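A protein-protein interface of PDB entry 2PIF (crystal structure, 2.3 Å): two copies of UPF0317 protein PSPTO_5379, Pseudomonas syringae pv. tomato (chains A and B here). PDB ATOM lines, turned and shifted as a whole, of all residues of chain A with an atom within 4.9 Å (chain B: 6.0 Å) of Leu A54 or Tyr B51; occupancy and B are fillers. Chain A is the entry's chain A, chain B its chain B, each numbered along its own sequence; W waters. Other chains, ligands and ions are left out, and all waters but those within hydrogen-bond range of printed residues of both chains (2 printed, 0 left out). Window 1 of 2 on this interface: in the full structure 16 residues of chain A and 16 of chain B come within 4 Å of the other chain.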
ATOM      1  N   ARG A  47      14.187  -6.747  23.882  1.00  0.00           N
ATOM      2  CA  ARG A  47      12.777  -6.434  23.681  1.00  0.00           C
ATOM      3  C   ARG A  47      12.008  -7.554  22.978  1.00  0.00           C
ATOM      4  O   ARG A  47      10.957  -7.974  23.453  1.00  0.00           O
ATOM      5  CB  ARG A  47      12.632  -5.137  22.883  1.00  0.00           C
ATOM      6  CG  ARG A  47      11.189  -4.753  22.628  1.00  0.00           C
ATOM      7  CD  ARG A  47      11.100  -3.420  21.921  1.00  0.00           C
ATOM      8  NE  ARG A  47       9.718  -2.990  21.738  1.00  0.00           N
ATOM      9  CZ  ARG A  47       8.869  -3.532  20.875  1.00  0.00           C
ATOM     10  NH1 ARG A  47       9.253  -4.534  20.099  1.00  0.00           N
ATOM     11  NH2 ARG A  47       7.631  -3.070  20.790  1.00  0.00           N
ATOM     12  N   ALA A  50      11.299 -10.089  25.196  1.00  0.00           N
ATOM     13  CA  ALA A  50      10.623  -9.513  26.352  1.00  0.00           C
ATOM     14  C   ALA A  50       9.101  -9.628  26.220  1.00  0.00           C
ATOM     15  O   ALA A  50       8.390  -9.656  27.224  1.00  0.00           O
ATOM     16  CB  ALA A  50      11.043  -8.057  26.543  1.00  0.00           C
ATOM     17  N   TYR A  51       8.605  -9.691  24.984  1.00  0.00           N
ATOM     18  CA  TYR A  51       7.172  -9.842  24.768  1.00  0.00           C
ATOM     19  C   TYR A  51       6.782 -11.240  25.217  1.00  0.00           C
ATOM     20  O   TYR A  51       5.734 -11.435  25.830  1.00  0.00           O
ATOM     21  CB  TYR A  51       6.781  -9.702  23.292  1.00  0.00           C
ATOM     22  CG  TYR A  51       5.303  -9.981  23.087  1.00  0.00           C
ATOM     23  CD1 TYR A  51       4.338  -9.047  23.468  1.00  0.00           C
ATOM     24  CD2 TYR A  51       4.869 -11.212  22.606  1.00  0.00           C
ATOM     25  CE1 TYR A  51       2.973  -9.332  23.380  1.00  0.00           C
ATOM     26  CE2 TYR A  51       3.505 -11.514  22.515  1.00  0.00           C
ATOM     27  CZ  TYR A  51       2.563 -10.566  22.906  1.00  0.00           C
ATOM     28  OH  TYR A  51       1.217 -10.862  22.833  1.00  0.00           O
ATOM     29  N   ASP A  52       7.621 -12.217  24.876  1.00  0.00           N
ATOM     30  CA  ASP A  52       7.364 -13.601  25.261  1.00  0.00           C
ATOM     31  C   ASP A  52       7.318 -13.703  26.775  1.00  0.00           C
ATOM     32  O   ASP A  52       6.416 -14.341  27.339  1.00  0.00           O
ATOM     33  CB  ASP A  52       8.467 -14.541  24.754  1.00  0.00           C
ATOM     34  CG  ASP A  52       8.536 -14.617  23.240  1.00  0.00           C
ATOM     35  OD1 ASP A  52       8.225 -15.693  22.674  1.00  0.00           O
ATOM     36  OD2 ASP A  52       8.903 -13.600  22.617  1.00  0.00           O
ATOM     37  N   PHE A  53       8.281 -13.079  27.448  1.00  0.00           N
ATOM     38  CA  PHE A  53       8.281 -13.190  28.898  1.00  0.00           C
ATOM     39  C   PHE A  53       7.191 -12.370  29.597  1.00  0.00           C
ATOM     40  O   PHE A  53       6.665 -12.797  30.614  1.00  0.00           O
ATOM     41  CB  PHE A  53       9.648 -12.835  29.495  1.00  0.00           C
ATOM     42  CG  PHE A  53       9.695 -13.005  30.989  1.00  0.00           C
ATOM     43  CD1 PHE A  53       9.614 -14.277  31.551  1.00  0.00           C
ATOM     44  CD2 PHE A  53       9.726 -11.896  31.832  1.00  0.00           C
ATOM     45  CE1 PHE A  53       9.553 -14.454  32.925  1.00  0.00           C
ATOM     46  CE2 PHE A  53       9.667 -12.048  33.215  1.00  0.00           C
ATOM     47  CZ  PHE A  53       9.577 -13.341  33.765  1.00  0.00           C
ATOM     48  N   LEU A  54       6.848 -11.207  29.060  1.00  0.00           N
ATOM     49  CA  LEU A  54       5.810 -10.386  29.678  1.00  0.00           C
ATOM     50  C   LEU A  54       4.521 -11.200  29.704  1.00  0.00           C
ATOM     51  O   LEU A  54       3.798 -11.204  30.705  1.00  0.00           O
ATOM     52  CB  LEU A  54       5.604  -9.077  28.897  1.00  0.00           C
ATOM     53  CG  LEU A  54       4.696  -7.991  29.508  1.00  0.00           C
ATOM     54  CD1 LEU A  54       5.045  -7.751  30.977  1.00  0.00           C
ATOM     55  CD2 LEU A  54       4.858  -6.697  28.712  1.00  0.00           C
ATOM     56  N   LEU A  55       4.268 -11.916  28.608  1.00  0.00           N
ATOM     57  CA  LEU A  55       3.069 -12.743  28.493  1.00  0.00           C
ATOM     58  C   LEU A  55       3.199 -13.989  29.350  1.00  0.00           C
ATOM     59  O   LEU A  55       2.203 -14.517  29.863  1.00  0.00           O
ATOM     60  CB  LEU A  55       2.820 -13.151  27.035  1.00  0.00           C
ATOM     61  CG  LEU A  55       1.612 -14.058  26.758  1.00  0.00           C
ATOM     62  CD1 LEU A  55       0.330 -13.397  27.242  1.00  0.00           C
ATOM     63  CD2 LEU A  55       1.525 -14.340  25.252  1.00  0.00           C
ATOM     64  N   TYR A  56       4.434 -14.458  29.497  1.00  0.00           N
ATOM     65  CA  TYR A  56       4.709 -15.634  30.297  1.00  0.00           C
ATOM     66  C   TYR A  56       4.378 -15.202  31.717  1.00  0.00           C
ATOM     67  O   TYR A  56       3.817 -15.980  32.513  1.00  0.00           O
ATOM     68  CB  TYR A  56       6.185 -16.010  30.164  1.00  0.00           C
ATOM     69  CG  TYR A  56       6.548 -17.387  30.679  1.00  0.00           C
ATOM     70  CD1 TYR A  56       6.220 -18.540  29.967  1.00  0.00           C
ATOM     71  CD2 TYR A  56       7.259 -17.535  31.861  1.00  0.00           C
ATOM     72  CE1 TYR A  56       6.604 -19.813  30.423  1.00  0.00           C
ATOM     73  CE2 TYR A  56       7.644 -18.802  32.327  1.00  0.00           C
ATOM     74  CZ  TYR A  56       7.317 -19.926  31.604  1.00  0.00           C
ATOM     75  OH  TYR A  56       7.725 -21.155  32.060  1.00  0.00           O
ATOM     76  N   ALA A  57       4.703 -13.947  32.025  1.00  0.00           N
ATOM     77  CA  ALA A  57       4.425 -13.418  33.348  1.00  0.00           C
ATOM     78  C   ALA A  57       2.927 -13.165  33.542  1.00  0.00           C
ATOM     79  O   ALA A  57       2.407 -13.373  34.636  1.00  0.00           O
ATOM     80  CB  ALA A  57       5.214 -12.142  33.593  1.00  0.00           C
ATOM     81  N   GLN A  58       2.222 -12.724  32.502  1.00  0.00           N
ATOM     82  CA  GLN A  58       0.795 -12.489  32.688  1.00  0.00           C
ATOM     83  C   GLN A  58       0.082 -13.828  32.755  1.00  0.00           C
ATOM     84  O   GLN A  58      -0.957 -13.951  33.393  1.00  0.00           O
ATOM     85  CB  GLN A  58       0.218 -11.580  31.587  1.00  0.00           C
ATOM     86  CG  GLN A  58      -0.316 -12.250  30.327  1.00  0.00           C
ATOM     87  CD  GLN A  58      -1.765 -12.715  30.452  1.00  0.00           C
ATOM     88  OE1 GLN A  58      -2.544 -12.211  31.268  1.00  0.00           O
ATOM     89  NE2 GLN A  58      -2.135 -13.668  29.616  1.00  0.00           N
ATOM     90  N   ILE A  66       5.445  -9.831  38.687  1.00  0.00           N
ATOM     91  CA  ILE A  66       6.258  -8.685  38.317  1.00  0.00           C
ATOM     92  C   ILE A  66       6.198  -7.523  39.323  1.00  0.00           C
ATOM     93  O   ILE A  66       5.110  -7.079  39.712  1.00  0.00           O
ATOM     94  CB  ILE A  66       5.820  -8.143  36.942  1.00  0.00           C
ATOM     95  CG1 ILE A  66       6.100  -9.177  35.848  1.00  0.00           C
ATOM     96  CG2 ILE A  66       6.556  -6.855  36.631  1.00  0.00           C
ATOM     97  CD1 ILE A  66       5.834  -8.653  34.444  1.00  0.00           C
ATOM     98  N   VAL A  69       8.960  -3.436  35.373  1.00  0.00           N
ATOM     99  CA  VAL A  69       9.517  -3.713  34.064  1.00  0.00           C
ATOM    100  C   VAL A  69      10.131  -2.409  33.606  1.00  0.00           C
ATOM    101  O   VAL A  69       9.434  -1.400  33.496  1.00  0.00           O
ATOM    102  CB  VAL A  69       8.430  -4.067  33.054  1.00  0.00           C
ATOM    103  CG1 VAL A  69       9.080  -4.516  31.734  1.00  0.00           C
ATOM    104  CG2 VAL A  69       7.492  -5.128  33.647  1.00  0.00           C
ATOM    105  N   SER A  70      11.432  -2.428  33.329  1.00  0.00           N
ATOM    106  CA  SER A  70      12.136  -1.229  32.881  1.00  0.00           C
ATOM    107  C   SER A  70      11.761  -0.919  31.440  1.00  0.00           C
ATOM    108  O   SER A  70      11.207  -1.762  30.744  1.00  0.00           O
ATOM    109  CB  SER A  70      13.653  -1.447  32.975  1.00  0.00           C
ATOM    110  OG  SER A  70      14.099  -2.357  31.973  1.00  0.00           O
ATOM    111  N   VAL A 118      15.337  -5.402  28.050  1.00  0.00           N
ATOM    112  CA  VAL A 118      14.211  -5.116  28.927  1.00  0.00           C
ATOM    113  C   VAL A 118      14.416  -5.858  30.230  1.00  0.00           C
ATOM    114  O   VAL A 118      14.531  -7.085  30.235  1.00  0.00           O
ATOM    115  CB  VAL A 118      12.862  -5.553  28.304  1.00  0.00           C
ATOM    116  CG1 VAL A 118      11.763  -5.498  29.358  1.00  0.00           C
ATOM    117  CG2 VAL A 118      12.496  -4.623  27.147  1.00  0.00           C
ATOM    118  N   PHE A 120      13.195  -7.132  33.929  1.00  0.00           N
ATOM    119  CA  PHE A 120      12.006  -7.515  34.682  1.00  0.00           C
ATOM    120  C   PHE A 120      12.406  -7.809  36.136  1.00  0.00           C
ATOM    121  O   PHE A 120      13.199  -8.715  36.382  1.00  0.00           O
ATOM    122  CB  PHE A 120      11.392  -8.774  34.071  1.00  0.00           C
ATOM    123  CG  PHE A 120      10.831  -8.585  32.673  1.00  0.00           C
ATOM    124  CD1 PHE A 120       9.482  -8.274  32.484  1.00  0.00           C
ATOM    125  CD2 PHE A 120      11.626  -8.792  31.551  1.00  0.00           C
ATOM    126  CE1 PHE A 120       8.942  -8.186  31.206  1.00  0.00           C
ATOM    127  CE2 PHE A 120      11.090  -8.700  30.267  1.00  0.00           C
ATOM    128  CZ  PHE A 120       9.744  -8.398  30.098  1.00  0.00           C
ATOM    129  N   PRO B  46      -0.957  -5.727  16.218  1.00  0.00           N
ATOM    130  CA  PRO B  46       0.097  -6.514  15.583  1.00  0.00           C
ATOM    131  C   PRO B  46       1.117  -6.783  16.685  1.00  0.00           C
ATOM    132  O   PRO B  46       1.370  -5.915  17.528  1.00  0.00           O
ATOM    133  CB  PRO B  46       0.622  -5.568  14.511  1.00  0.00           C
ATOM    134  CG  PRO B  46      -0.615  -4.814  14.114  1.00  0.00           C
ATOM    135  CD  PRO B  46      -1.200  -4.486  15.462  1.00  0.00           C
ATOM    136  N   ARG B  47       1.691  -7.981  16.690  1.00  0.00           N
ATOM    137  CA  ARG B  47       2.654  -8.352  17.723  1.00  0.00           C
ATOM    138  C   ARG B  47       3.584  -7.231  18.164  1.00  0.00           C
ATOM    139  O   ARG B  47       3.780  -7.035  19.361  1.00  0.00           O
ATOM    140  CB  ARG B  47       3.495  -9.552  17.282  1.00  0.00           C
ATOM    141  CG  ARG B  47       4.444 -10.027  18.380  1.00  0.00           C
ATOM    142  CD  ARG B  47       5.044 -11.389  18.084  1.00  0.00           C
ATOM    143  NE  ARG B  47       5.925 -11.820  19.165  1.00  0.00           N
ATOM    144  CZ  ARG B  47       7.104 -11.268  19.435  1.00  0.00           C
ATOM    145  NH1 ARG B  47       7.552 -10.264  18.699  1.00  0.00           N
ATOM    146  NH2 ARG B  47       7.831 -11.716  20.445  1.00  0.00           N
ATOM    147  N   ASP B  48       4.147  -6.495  17.207  1.00  0.00           N
ATOM    148  CA  ASP B  48       5.068  -5.418  17.545  1.00  0.00           C
ATOM    149  C   ASP B  48       4.459  -4.369  18.472  1.00  0.00           C
ATOM    150  O   ASP B  48       5.139  -3.854  19.359  1.00  0.00           O
ATOM    151  CB  ASP B  48       5.598  -4.735  16.282  1.00  0.00           C
ATOM    152  CG  ASP B  48       6.664  -3.694  16.593  1.00  0.00           C
ATOM    153  OD1 ASP B  48       6.454  -2.498  16.294  1.00  0.00           O
ATOM    154  OD2 ASP B  48       7.718  -4.074  17.149  1.00  0.00           O
ATOM    155  N   TRP B  49       3.187  -4.042  18.274  1.00  0.00           N
ATOM    156  CA  TRP B  49       2.546  -3.056  19.134  1.00  0.00           C
ATOM    157  C   TRP B  49       1.903  -3.731  20.325  1.00  0.00           C
ATOM    158  O   TRP B  49       1.566  -3.086  21.314  1.00  0.00           O
ATOM    159  CB  TRP B  49       1.494  -2.247  18.369  1.00  0.00           C
ATOM    160  CG  TRP B  49       2.090  -1.120  17.606  1.00  0.00           C
ATOM    161  CD1 TRP B  49       2.645  -1.171  16.359  1.00  0.00           C
ATOM    162  CD2 TRP B  49       2.260   0.225  18.071  1.00  0.00           C
ATOM    163  NE1 TRP B  49       3.152   0.062  16.019  1.00  0.00           N
ATOM    164  CE2 TRP B  49       2.930   0.934  17.050  1.00  0.00           C
ATOM    165  CE3 TRP B  49       1.914   0.898  19.253  1.00  0.00           C
ATOM    166  CZ2 TRP B  49       3.260   2.291  17.178  1.00  0.00           C
ATOM    167  CZ3 TRP B  49       2.242   2.246  19.379  1.00  0.00           C
ATOM    168  CH2 TRP B  49       2.908   2.928  18.347  1.00  0.00           C
ATOM    169  N   ALA B  50       1.729  -5.041  20.223  1.00  0.00           N
ATOM    170  CA  ALA B  50       1.129  -5.799  21.307  1.00  0.00           C
ATOM    171  C   ALA B  50       2.041  -5.693  22.531  1.00  0.00           C
ATOM    172  O   ALA B  50       1.552  -5.710  23.662  1.00  0.00           O
ATOM    173  CB  ALA B  50       0.939  -7.253  20.896  1.00  0.00           C
ATOM    174  N   TYR B  51       3.355  -5.570  22.314  1.00  0.00           N
ATOM    175  CA  TYR B  51       4.282  -5.432  23.451  1.00  0.00           C
ATOM    176  C   TYR B  51       3.987  -4.135  24.202  1.00  0.00           C
ATOM    177  O   TYR B  51       3.880  -4.136  25.420  1.00  0.00           O
ATOM    178  CB  TYR B  51       5.748  -5.390  23.018  1.00  0.00           C
ATOM    179  CG  TYR B  51       6.664  -5.162  24.204  1.00  0.00           C
ATOM    180  CD1 TYR B  51       6.982  -6.206  25.069  1.00  0.00           C
ATOM    181  CD2 TYR B  51       7.142  -3.885  24.516  1.00  0.00           C
ATOM    182  CE1 TYR B  51       7.749  -5.990  26.222  1.00  0.00           C
ATOM    183  CE2 TYR B  51       7.904  -3.660  25.668  1.00  0.00           C
ATOM    184  CZ  TYR B  51       8.198  -4.722  26.511  1.00  0.00           C
ATOM    185  OH  TYR B  51       8.927  -4.529  27.652  1.00  0.00           O
ATOM    186  N   ASP B  52       3.874  -3.035  23.460  1.00  0.00           N
ATOM    187  CA  ASP B  52       3.568  -1.720  24.028  1.00  0.00           C
ATOM    188  C   ASP B  52       2.278  -1.732  24.843  1.00  0.00           C
ATOM    189  O   ASP B  52       2.223  -1.172  25.937  1.00  0.00           O
ATOM    190  CB  ASP B  52       3.415  -0.686  22.914  1.00  0.00           C
ATOM    191  CG  ASP B  52       4.709  -0.416  22.185  1.00  0.00           C
ATOM    192  OD1 ASP B  52       5.464   0.483  22.618  1.00  0.00           O
ATOM    193  OD2 ASP B  52       4.974  -1.113  21.180  1.00  0.00           O
ATOM    194  N   PHE B  53       1.236  -2.362  24.311  1.00  0.00           N
ATOM    195  CA  PHE B  53      -0.045  -2.407  25.018  1.00  0.00           C
ATOM    196  C   PHE B  53      -0.053  -3.354  26.225  1.00  0.00           C
ATOM    197  O   PHE B  53      -0.598  -3.020  27.283  1.00  0.00           O
ATOM    198  CB  PHE B  53      -1.188  -2.796  24.073  1.00  0.00           C
ATOM    199  CG  PHE B  53      -2.527  -2.855  24.756  1.00  0.00           C
ATOM    200  CD1 PHE B  53      -3.166  -1.691  25.159  1.00  0.00           C
ATOM    201  CD2 PHE B  53      -3.112  -4.079  25.061  1.00  0.00           C
ATOM    202  CE1 PHE B  53      -4.371  -1.739  25.864  1.00  0.00           C
ATOM    203  CE2 PHE B  53      -4.315  -4.148  25.761  1.00  0.00           C
ATOM    204  CZ  PHE B  53      -4.949  -2.973  26.166  1.00  0.00           C
ATOM    205  N   LEU B  54       0.523  -4.542  26.065  1.00  0.00           N
ATOM    206  CA  LEU B  54       0.580  -5.484  27.181  1.00  0.00           C
ATOM    207  C   LEU B  54       1.295  -4.773  28.346  1.00  0.00           C
ATOM    208  O   LEU B  54       0.874  -4.895  29.499  1.00  0.00           O
ATOM    209  CB  LEU B  54       1.326  -6.764  26.761  1.00  0.00           C
ATOM    210  CG  LEU B  54       1.476  -7.938  27.742  1.00  0.00           C
ATOM    211  CD1 LEU B  54       0.124  -8.396  28.284  1.00  0.00           C
ATOM    212  CD2 LEU B  54       2.174  -9.085  27.022  1.00  0.00           C
ATOM    213  N   LEU B  55       2.352  -4.011  28.036  1.00  0.00           N
ATOM    214  CA  LEU B  55       3.108  -3.276  29.057  1.00  0.00           C
ATOM    215  C   LEU B  55       2.268  -2.106  29.569  1.00  0.00           C
ATOM    216  O   LEU B  55       2.393  -1.693  30.727  1.00  0.00           O
ATOM    217  CB  LEU B  55       4.425  -2.735  28.487  1.00  0.00           C
ATOM    218  CG  LEU B  55       5.288  -1.864  29.416  1.00  0.00           C
ATOM    219  CD1 LEU B  55       5.737  -2.685  30.611  1.00  0.00           C
ATOM    220  CD2 LEU B  55       6.516  -1.330  28.674  1.00  0.00           C
ATOM    221  N   TYR B  56       1.418  -1.571  28.697  1.00  0.00           N
ATOM    222  CA  TYR B  56       0.548  -0.463  29.066  1.00  0.00           C
ATOM    223  C   TYR B  56      -0.429  -1.014  30.096  1.00  0.00           C
ATOM    224  O   TYR B  56      -0.771  -0.353  31.070  1.00  0.00           O
ATOM    225  CB  TYR B  56      -0.199   0.045  27.830  1.00  0.00           C
ATOM    226  CG  TYR B  56      -0.922   1.377  27.977  1.00  0.00           C
ATOM    227  CD1 TYR B  56      -0.243   2.536  28.353  1.00  0.00           C
ATOM    228  CD2 TYR B  56      -2.274   1.488  27.656  1.00  0.00           C
ATOM    229  CE1 TYR B  56      -0.893   3.775  28.401  1.00  0.00           C
ATOM    230  CE2 TYR B  56      -2.940   2.719  27.699  1.00  0.00           C
ATOM    231  CZ  TYR B  56      -2.243   3.854  28.071  1.00  0.00           C
ATOM    232  OH  TYR B  56      -2.907   5.054  28.111  1.00  0.00           O
ATOM    233  N   GLN B  58       0.057  -3.790  32.106  1.00  0.00           N
ATOM    234  CA  GLN B  58       0.709  -4.140  33.356  1.00  0.00           C
ATOM    235  C   GLN B  58       0.988  -2.888  34.182  1.00  0.00           C
ATOM    236  O   GLN B  58       1.041  -2.952  35.410  1.00  0.00           O
ATOM    237  CB  GLN B  58       1.991  -4.955  33.100  1.00  0.00           C
ATOM    238  CG  GLN B  58       3.337  -4.216  33.192  1.00  0.00           C
ATOM    239  CD  GLN B  58       3.771  -3.885  34.616  1.00  0.00           C
ATOM    240  OE1 GLN B  58       3.357  -4.531  35.579  1.00  0.00           O
ATOM    241  NE2 GLN B  58       4.622  -2.885  34.746  1.00  0.00           N
ATOM    242  N   PHE B 120      -6.573  -8.760  22.774  1.00  0.00           N
ATOM    243  CA  PHE B 120      -6.624  -8.464  24.190  1.00  0.00           C
ATOM    244  C   PHE B 120      -8.055  -8.259  24.640  1.00  0.00           C
ATOM    245  O   PHE B 120      -8.697  -7.280  24.253  1.00  0.00           O
ATOM    246  CB  PHE B 120      -5.848  -7.185  24.489  1.00  0.00           C
ATOM    247  CG  PHE B 120      -4.367  -7.322  24.341  1.00  0.00           C
ATOM    248  CD1 PHE B 120      -3.566  -7.559  25.449  1.00  0.00           C
ATOM    249  CD2 PHE B 120      -3.768  -7.180  23.101  1.00  0.00           C
ATOM    250  CE1 PHE B 120      -2.182  -7.648  25.325  1.00  0.00           C
ATOM    251  CE2 PHE B 120      -2.381  -7.269  22.964  1.00  0.00           C
ATOM    252  CZ  PHE B 120      -1.588  -7.500  24.074  1.00  0.00           C
ATOM    253  N   GLY B 161       6.239   2.189  26.458  1.00  0.00           N
ATOM    254  CA  GLY B 161       6.777   2.139  25.115  1.00  0.00           C
ATOM    255  C   GLY B 161       6.348   3.351  24.305  1.00  0.00           C
ATOM    256  O   GLY B 161       6.656   4.487  24.670  1.00  0.00           O
HETATM  257  O   HOH W   1       6.515  -1.314  34.460  1.00  0.00           O
HETATM  258  O   HOH W   2       9.897  -2.197  28.215  1.00  0.00           O
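Leu A54 touches three residues of chain B.
Tyr B51 touches five residues of chain A.
Printed residues of chain A within 4 Å of Leu B55: Leu A54 (3.7 Å) and Val A69 (3.9 Å).
Of the printed residues of chain A, Asp B48 touches Arg A47.
Of the printed residues of chain A, Leu B54 touches Tyr A51 (3.7 Å), Leu A54 (3.7 Å) and Leu A55 (3.9 Å).
Gly B161 touches none of the printed residues of chain A.
Ser A70 touches none of the printed residues of chain B.
NH2 of Arg A47 lies within salt-bridge range of OD2 of Asp B52.
The side-chain carboxylate (OD2) of Asp A52 lies within salt-bridge range of the guanidinium group (NH2) of Arg B47 (3.1 Å).
The guanidinium group (NH1) of Arg A47 is in salt-bridge range of the side-chain carboxylate (OD2) of Asp B48 (3.4 Å).
Printed residues of chain B that touch a printed residue of chain A: Arg B47, Asp B48, Ala B50, Tyr B51, Asp B52, Leu B54, Leu B55 and Gln B58.
Hydrophobic or aromatic side chains of chain B that line the printed part of chain A: Ala B50, Tyr B51, Leu B54 and Leu B55.
Of the 15 printed residues of chain A, 8 touch a printed residue of chain B.
Among the printed residues, 16 pairs touch across the chains.
Among the printed residues, Asp or Glu carboxylates within 4 Å of a Lys or Arg side-chain nitrogen of the other chain: Arg A47 with Asp B48, Arg A47 with Asp B52 and Asp A52 with Arg B47.
Arg A47 touches Tyr B51, and with the chains exchanged Tyr A51 touches Arg B47.
Arg A47 touches Asp B52, and with the chains exchanged Asp A52 touches Arg B47.
Ala A50 touches Tyr B51, and with the chains exchanged Tyr A51 touches Ala B50.
Tyr A51 touches Leu B54, and with the chains exchanged Leu A54 touches Tyr B51.
Positions printed for both chains: 47, 50, 51, 52, 53, 54, 55, 56, 58 and 120.
Of the 16 pairs that touch across the chains among the printed residues, 12 have their exchanged pair printed and touching as well.
Water W1 bridges NE2 of Gln B58 (2.5 Å) and O of Val A69 (3.1 Å).
Water W2 lies within hydrogen-bond range of OH of Tyr B51 (2.6 Å) and O of Ser A70 (2.9 Å).
NH2 of Arg A47 touches CB of Tyr B51, 3.7 Å away.
Ala A50 touches Tyr B51 (O to CE1, 3.9 Å).
Tyr A51 touches Arg B47 (CB to NH2, 3.6 Å).
Tyr A51 touches Ala B50 (CE1 to CB, 3.8 Å).
Tyr A51 touches Tyr B51 (CD1 to CA, 3.6 Å).
Tyr A51 touches Leu B54.
Leu A54 touches Leu B54 (CG to CG, 3.7 Å).
Leu B55 touches Leu A54 (N to CD2, 3.7 Å).
Leu B54 touches Leu A55.
Val A69 touches Leu B55 (CB to CD1, 3.9 Å).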
